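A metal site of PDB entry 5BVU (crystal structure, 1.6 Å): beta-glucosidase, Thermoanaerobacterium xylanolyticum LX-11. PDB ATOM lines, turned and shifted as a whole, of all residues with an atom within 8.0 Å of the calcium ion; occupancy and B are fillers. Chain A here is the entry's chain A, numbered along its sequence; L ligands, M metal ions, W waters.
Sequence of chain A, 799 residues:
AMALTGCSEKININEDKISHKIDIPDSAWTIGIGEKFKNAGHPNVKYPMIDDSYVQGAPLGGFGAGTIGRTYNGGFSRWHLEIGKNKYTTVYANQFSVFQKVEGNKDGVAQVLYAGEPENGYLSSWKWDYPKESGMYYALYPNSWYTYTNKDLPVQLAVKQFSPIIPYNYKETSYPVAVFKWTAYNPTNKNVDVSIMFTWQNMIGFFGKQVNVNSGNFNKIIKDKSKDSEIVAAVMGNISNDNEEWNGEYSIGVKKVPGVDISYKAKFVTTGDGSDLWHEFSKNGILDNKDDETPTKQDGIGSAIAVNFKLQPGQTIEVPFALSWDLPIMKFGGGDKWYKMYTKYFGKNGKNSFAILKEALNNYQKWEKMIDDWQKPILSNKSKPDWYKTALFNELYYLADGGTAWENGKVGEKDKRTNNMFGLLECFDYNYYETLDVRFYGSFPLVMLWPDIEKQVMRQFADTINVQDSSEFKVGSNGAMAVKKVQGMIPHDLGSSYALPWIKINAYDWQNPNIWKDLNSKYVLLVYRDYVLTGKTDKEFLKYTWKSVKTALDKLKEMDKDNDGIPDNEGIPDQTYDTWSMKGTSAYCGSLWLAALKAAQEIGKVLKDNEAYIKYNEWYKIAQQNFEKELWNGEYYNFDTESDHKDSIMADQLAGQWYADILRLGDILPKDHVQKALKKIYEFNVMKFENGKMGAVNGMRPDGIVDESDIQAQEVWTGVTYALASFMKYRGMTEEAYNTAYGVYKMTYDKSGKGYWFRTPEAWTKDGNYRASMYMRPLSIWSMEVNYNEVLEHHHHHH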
ATOM      1  N   LYS A 557      -5.372  34.669 -30.283  1.00  0.00           N
ATOM      2  CA  LYS A 557      -4.109  33.899 -30.277  1.00  0.00           C
ATOM      3  C   LYS A 557      -3.178  34.319 -29.136  1.00  0.00           C
ATOM      4  O   LYS A 557      -2.502  33.481 -28.566  1.00  0.00           O
ATOM      5  CB  LYS A 557      -3.399  34.040 -31.616  1.00  0.00           C
ATOM      6  CG  LYS A 557      -2.115  33.226 -31.778  1.00  0.00           C
ATOM      7  CD  LYS A 557      -2.356  31.734 -31.597  1.00  0.00           C
ATOM      8  CE  LYS A 557      -1.379  30.881 -32.400  1.00  0.00           C
ATOM      9  NZ  LYS A 557       0.029  31.037 -31.983  1.00  0.00           N
ATOM     10  N   MET A 559      -3.913  34.948 -26.212  1.00  0.00           N
ATOM     11  CA  MET A 559      -4.389  34.337 -24.967  1.00  0.00           C
ATOM     12  C   MET A 559      -3.983  32.871 -24.812  1.00  0.00           C
ATOM     13  O   MET A 559      -4.350  32.217 -23.838  1.00  0.00           O
ATOM     14  CB  MET A 559      -5.915  34.481 -24.865  1.00  0.00           C
ATOM     15  CG  MET A 559      -6.347  35.926 -24.740  1.00  0.00           C
ATOM     16  SD  MET A 559      -8.134  36.109 -24.866  1.00  0.00           S
ATOM     17  CE  MET A 559      -8.322  37.862 -24.620  1.00  0.00           C
ATOM     18  N   ASP A 560      -3.212  32.365 -25.762  1.00  0.00           N
ATOM     19  CA  ASP A 560      -2.568  31.066 -25.628  1.00  0.00           C
ATOM     20  C   ASP A 560      -1.362  31.199 -24.688  1.00  0.00           C
ATOM     21  O   ASP A 560      -0.316  31.666 -25.095  1.00  0.00           O
ATOM     22  CB  ASP A 560      -2.134  30.587 -27.003  1.00  0.00           C
ATOM     23  CG  ASP A 560      -1.359  29.284 -26.969  1.00  0.00           C
ATOM     24  OD1 ASP A 560      -1.436  28.554 -25.970  1.00  0.00           O
ATOM     25  OD2 ASP A 560      -0.672  29.016 -27.955  1.00  0.00           O
ATOM     26  N   LYS A 561      -1.518  30.773 -23.441  1.00  0.00           N
ATOM     27  CA  LYS A 561      -0.453  30.908 -22.420  1.00  0.00           C
ATOM     28  C   LYS A 561       0.662  29.876 -22.541  1.00  0.00           C
ATOM     29  O   LYS A 561       1.828  30.197 -22.317  1.00  0.00           O
ATOM     30  CB  LYS A 561      -1.054  30.809 -21.014  1.00  0.00           C
ATOM     31  CG  LYS A 561      -2.037  31.920 -20.654  1.00  0.00           C
ATOM     32  CD  LYS A 561      -1.359  33.277 -20.602  1.00  0.00           C
ATOM     33  CE  LYS A 561      -1.397  34.017 -21.935  1.00  0.00           C
ATOM     34  NZ  LYS A 561      -0.130  34.739 -22.202  1.00  0.00           N
ATOM     35  N   ASP A 562       0.315  28.642 -22.868  1.00  0.00           N
ATOM     36  CA  ASP A 562       1.272  27.536 -22.820  1.00  0.00           C
ATOM     37  C   ASP A 562       1.787  27.141 -24.201  1.00  0.00           C
ATOM     38  O   ASP A 562       2.389  26.092 -24.370  1.00  0.00           O
ATOM     39  CB  ASP A 562       0.631  26.340 -22.140  1.00  0.00           C
ATOM     40  CG  ASP A 562      -0.464  25.735 -22.961  1.00  0.00           C
ATOM     41  OD1 ASP A 562      -1.038  26.457 -23.809  1.00  0.00           O
ATOM     42  OD2 ASP A 562      -0.756  24.534 -22.771  1.00  0.00           O
ATOM     43  N   ASN A 563       1.520  27.986 -25.187  1.00  0.00           N
ATOM     44  CA  ASN A 563       1.953  27.792 -26.563  1.00  0.00           C
ATOM     45  C   ASN A 563       1.594  26.442 -27.216  1.00  0.00           C
ATOM     46  O   ASN A 563       2.377  25.874 -27.977  1.00  0.00           O
ATOM     47  CB  ASN A 563       3.449  28.081 -26.717  1.00  0.00           C
ATOM     48  CG  ASN A 563       3.737  28.971 -27.904  1.00  0.00           C
ATOM     49  OD1 ASN A 563       3.526  30.179 -27.832  1.00  0.00           O
ATOM     50  ND2 ASN A 563       4.169  28.388 -29.009  1.00  0.00           N
ATOM     51  N   ASP A 564       0.379  25.965 -26.943  1.00  0.00           N
ATOM     52  CA  ASP A 564      -0.145  24.781 -27.632  1.00  0.00           C
ATOM     53  C   ASP A 564      -0.978  25.179 -28.858  1.00  0.00           C
ATOM     54  O   ASP A 564      -1.588  24.322 -29.507  1.00  0.00           O
ATOM     55  CB  ASP A 564      -0.953  23.906 -26.661  1.00  0.00           C
ATOM     56  CG  ASP A 564      -2.317  24.492 -26.312  1.00  0.00           C
ATOM     57  OD1 ASP A 564      -2.565  25.675 -26.586  1.00  0.00           O
ATOM     58  OD2 ASP A 564      -3.145  23.765 -25.699  1.00  0.00           O
ATOM     59  N   GLY A 565      -1.017  26.476 -29.164  1.00  0.00           N
ATOM     60  CA  GLY A 565      -1.725  26.992 -30.341  1.00  0.00           C
ATOM     61  C   GLY A 565      -3.190  27.339 -30.105  1.00  0.00           C
ATOM     62  O   GLY A 565      -3.888  27.742 -31.033  1.00  0.00           O
ATOM     63  N   ILE A 566      -3.638  27.202 -28.857  1.00  0.00           N
ATOM     64  CA  ILE A 566      -5.058  27.364 -28.499  1.00  0.00           C
ATOM     65  C   ILE A 566      -5.180  28.364 -27.344  1.00  0.00           C
ATOM     66  O   ILE A 566      -4.440  28.272 -26.365  1.00  0.00           O
ATOM     67  CB  ILE A 566      -5.670  26.018 -28.049  1.00  0.00           C
ATOM     68  CG1 ILE A 566      -5.402  24.935 -29.101  1.00  0.00           C
ATOM     69  CG2 ILE A 566      -7.170  26.143 -27.768  1.00  0.00           C
ATOM     70  CD1 ILE A 566      -5.813  23.556 -28.663  1.00  0.00           C
ATOM     71  N   PRO A 567      -6.115  29.314 -27.447  1.00  0.00           N
ATOM     72  CA  PRO A 567      -6.338  30.183 -26.287  1.00  0.00           C
ATOM     73  C   PRO A 567      -6.662  29.381 -25.023  1.00  0.00           C
ATOM     74  O   PRO A 567      -7.348  28.344 -25.105  1.00  0.00           O
ATOM     75  CB  PRO A 567      -7.521  31.075 -26.712  1.00  0.00           C
ATOM     76  CG  PRO A 567      -8.168  30.330 -27.832  1.00  0.00           C
ATOM     77  CD  PRO A 567      -7.095  29.562 -28.519  1.00  0.00           C
ATOM     78  N   ASP A 568      -6.135  29.821 -23.886  1.00  0.00           N
ATOM     79  CA  ASP A 568      -6.338  29.150 -22.612  1.00  0.00           C
ATOM     80  C   ASP A 568      -7.487  29.753 -21.806  1.00  0.00           C
ATOM     81  O   ASP A 568      -7.471  30.932 -21.464  1.00  0.00           O
ATOM     82  CB  ASP A 568      -5.089  29.296 -21.729  1.00  0.00           C
ATOM     83  CG  ASP A 568      -3.946  28.443 -22.214  1.00  0.00           C
ATOM     84  OD1 ASP A 568      -3.400  28.710 -23.314  1.00  0.00           O
ATOM     85  OD2 ASP A 568      -3.579  27.505 -21.471  1.00  0.00           O
ATOM     86  N   ASN A 569      -8.468  28.925 -21.444  1.00  0.00           N
ATOM     87  CA  ASN A 569      -9.452  29.363 -20.462  1.00  0.00           C
ATOM     88  C   ASN A 569      -8.722  29.527 -19.121  1.00  0.00           C
ATOM     89  O   ASN A 569      -7.785  28.775 -18.838  1.00  0.00           O
ATOM     90  CB  ASN A 569     -10.615  28.381 -20.364  1.00  0.00           C
ATOM     91  CG  ASN A 569     -11.454  28.313 -21.643  1.00  0.00           C
ATOM     92  OD1 ASN A 569     -11.269  27.426 -22.482  1.00  0.00           O
ATOM     93  ND2 ASN A 569     -12.391  29.243 -21.789  1.00  0.00           N
ATOM     94  N   GLY A 584      -7.602  25.858 -19.015  1.00  0.00           N
ATOM     95  CA  GLY A 584      -6.729  25.223 -19.982  1.00  0.00           C
ATOM     96  C   GLY A 584      -7.376  25.217 -21.357  1.00  0.00           C
ATOM     97  O   GLY A 584      -7.963  26.228 -21.769  1.00  0.00           O
ATOM     98  N   THR A 585      -7.269  24.104 -22.055  1.00  0.00           N
ATOM     99  CA  THR A 585      -7.928  23.956 -23.349  1.00  0.00           C
ATOM    100  C   THR A 585      -9.281  23.325 -23.065  1.00  0.00           C
ATOM    101  O   THR A 585      -9.354  22.278 -22.441  1.00  0.00           O
ATOM    102  CB  THR A 585      -7.127  23.058 -24.310  1.00  0.00           C
ATOM    103  OG1 THR A 585      -5.887  23.700 -24.647  1.00  0.00           O
ATOM    104  CG2 THR A 585      -7.891  22.823 -25.599  1.00  0.00           C
ATOM    105  N   TRP A 593     -12.527  27.711 -31.738  1.00  0.00           N
ATOM    106  CA  TRP A 593     -11.273  28.246 -32.279  1.00  0.00           C
ATOM    107  C   TRP A 593     -10.832  27.540 -33.571  1.00  0.00           C
ATOM    108  O   TRP A 593     -10.510  28.184 -34.566  1.00  0.00           O
ATOM    109  CB  TRP A 593     -10.204  28.146 -31.178  1.00  0.00           C
ATOM    110  CG  TRP A 593      -8.773  28.480 -31.554  1.00  0.00           C
ATOM    111  CD1 TRP A 593      -7.699  27.632 -31.508  1.00  0.00           C
ATOM    112  CD2 TRP A 593      -8.244  29.763 -31.918  1.00  0.00           C
ATOM    113  NE1 TRP A 593      -6.547  28.295 -31.847  1.00  0.00           N
ATOM    114  CE2 TRP A 593      -6.855  29.605 -32.110  1.00  0.00           C
ATOM    115  CE3 TRP A 593      -8.807  31.023 -32.125  1.00  0.00           C
ATOM    116  CZ2 TRP A 593      -6.026  30.662 -32.508  1.00  0.00           C
ATOM    117  CZ3 TRP A 593      -7.995  32.071 -32.508  1.00  0.00           C
ATOM    118  CH2 TRP A 593      -6.605  31.874 -32.683  1.00  0.00           C
ATOM    119  N   ASN A 626      -3.035  19.406 -31.318  1.00  0.00           N
ATOM    120  CA  ASN A 626      -3.012  19.508 -29.873  1.00  0.00           C
ATOM    121  C   ASN A 626      -4.367  19.367 -29.209  1.00  0.00           C
ATOM    122  O   ASN A 626      -4.472  18.815 -28.109  1.00  0.00           O
ATOM    123  CB  ASN A 626      -2.324  20.812 -29.476  1.00  0.00           C
ATOM    124  CG  ASN A 626      -0.842  20.774 -29.734  1.00  0.00           C
ATOM    125  OD1 ASN A 626      -0.255  19.694 -29.713  1.00  0.00           O
ATOM    126  ND2 ASN A 626      -0.235  21.914 -29.972  1.00  0.00           N
ATOM    127  N   GLU A 630      -4.864  16.542 -26.387  1.00  0.00           N
ATOM    128  CA  GLU A 630      -5.233  16.976 -25.046  1.00  0.00           C
ATOM    129  C   GLU A 630      -6.584  16.450 -24.567  1.00  0.00           C
ATOM    130  O   GLU A 630      -6.763  16.215 -23.377  1.00  0.00           O
ATOM    131  CB  GLU A 630      -5.230  18.503 -24.964  1.00  0.00           C
ATOM    132  CG  GLU A 630      -3.835  19.115 -25.086  1.00  0.00           C
ATOM    133  CD  GLU A 630      -3.867  20.584 -25.424  1.00  0.00           C
ATOM    134  OE1 GLU A 630      -4.966  21.196 -25.355  1.00  0.00           O
ATOM    135  OE2 GLU A 630      -2.803  21.128 -25.781  1.00  0.00           O
ATOM    136  N   THR A 641      -8.822  20.639 -19.980  1.00  0.00           N
ATOM    137  CA  THR A 641      -7.558  19.995 -19.558  1.00  0.00           C
ATOM    138  C   THR A 641      -7.202  20.159 -18.079  1.00  0.00           C
ATOM    139  O   THR A 641      -6.393  19.379 -17.560  1.00  0.00           O
ATOM    140  CB  THR A 641      -6.366  20.488 -20.397  1.00  0.00           C
ATOM    141  OG1 THR A 641      -6.276  21.924 -20.332  1.00  0.00           O
ATOM    142  CG2 THR A 641      -6.503  20.054 -21.850  1.00  0.00           C
ATOM    143  N   GLU A 642      -7.774  21.158 -17.385  1.00  0.00           N
ATOM    144  CA  GLU A 642      -7.289  21.531 -16.052  1.00  0.00           C
ATOM    145  C   GLU A 642      -8.310  21.668 -14.909  1.00  0.00           C
ATOM    146  O   GLU A 642      -7.918  21.773 -13.750  1.00  0.00           O
ATOM    147  CB  GLU A 642      -6.479  22.832 -16.147  1.00  0.00           C
ATOM    148  CG  GLU A 642      -5.175  22.663 -16.928  1.00  0.00           C
ATOM    149  CD  GLU A 642      -4.399  23.948 -17.040  1.00  0.00           C
ATOM    150  OE1 GLU A 642      -4.357  24.712 -16.055  1.00  0.00           O
ATOM    151  OE2 GLU A 642      -3.819  24.219 -18.117  1.00  0.00           O
HETATM  152  C1  LIG L   1      -2.993  21.952 -22.419  1.00  0.00           C
HETATM  153  O1  LIG L   1      -2.456  20.782 -21.789  1.00  0.00           O
HETATM  154  C2  LIG L   1      -3.124  23.076 -21.403  1.00  0.00           C
HETATM  155  O2  LIG L   1      -3.809  22.613 -20.230  1.00  0.00           O
HETATM  156  C3  LIG L   1      -3.901  24.252 -21.993  1.00  0.00           C
HETATM  157  O3  LIG L   1      -3.225  24.910 -23.077  1.00  0.00           O
HETATM  158 CA    CA M   1      -2.997  27.226 -24.970  1.00  0.00          CA
HETATM  159  O   HOH W   1      -5.149  26.215 -24.269  1.00  0.00           O
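ND2 of Asn 626 is in hydrogen-bond range of O of Asp 564 (2.8 Å). The backbone carbonyl oxygen (O) of Met 559 sits at hydrogen-bond distance from the backbone NH (N) of Asp 568 (3.0 Å). N of Asn 563 lies close to OD1 of Asp 560 (3.1 Å). The side-chain carboxylate (OD1) of Asp 568 lies close to the backbone NH (N) of Lys 561. The side-chain carboxylate of Asp 564 is in hydrogen-bond range of the side-chain hydroxyl of Thr 585, 2.9 Å away. OE2 of Glu 630 sits close to OD2 of Asp 564 (2.7 Å). The backbone NH (N) of Gly 565 is in hydrogen-bond range of the side-chain carboxylate (OD2) of Asp 560 (2.8 Å).
Along chain A the residues within 4 Å of the calcium ion span positions 560 to 568.
OD1 of Asp 568 binds the calcium ion (2.3 Å). The backbone carbonyl oxygen (O) of Ile 566 binds the calcium ion (2.3 Å). OD1 of Asp 560 binds the calcium ion, 2.3 Å away. The side-chain carboxylate (OD1) of Asp 564 is bound to the calcium ion (2.3 Å). The calcium ion is bound by OD1 of Asp 562, 2.4 Å away. The calcium ion is bound by water W1, 2.5 Å away. The calcium ion has six donor atoms within binding distance. Slightly farther from the calcium ion lies an oxygen (O3) of the ligand (3.0 Å).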
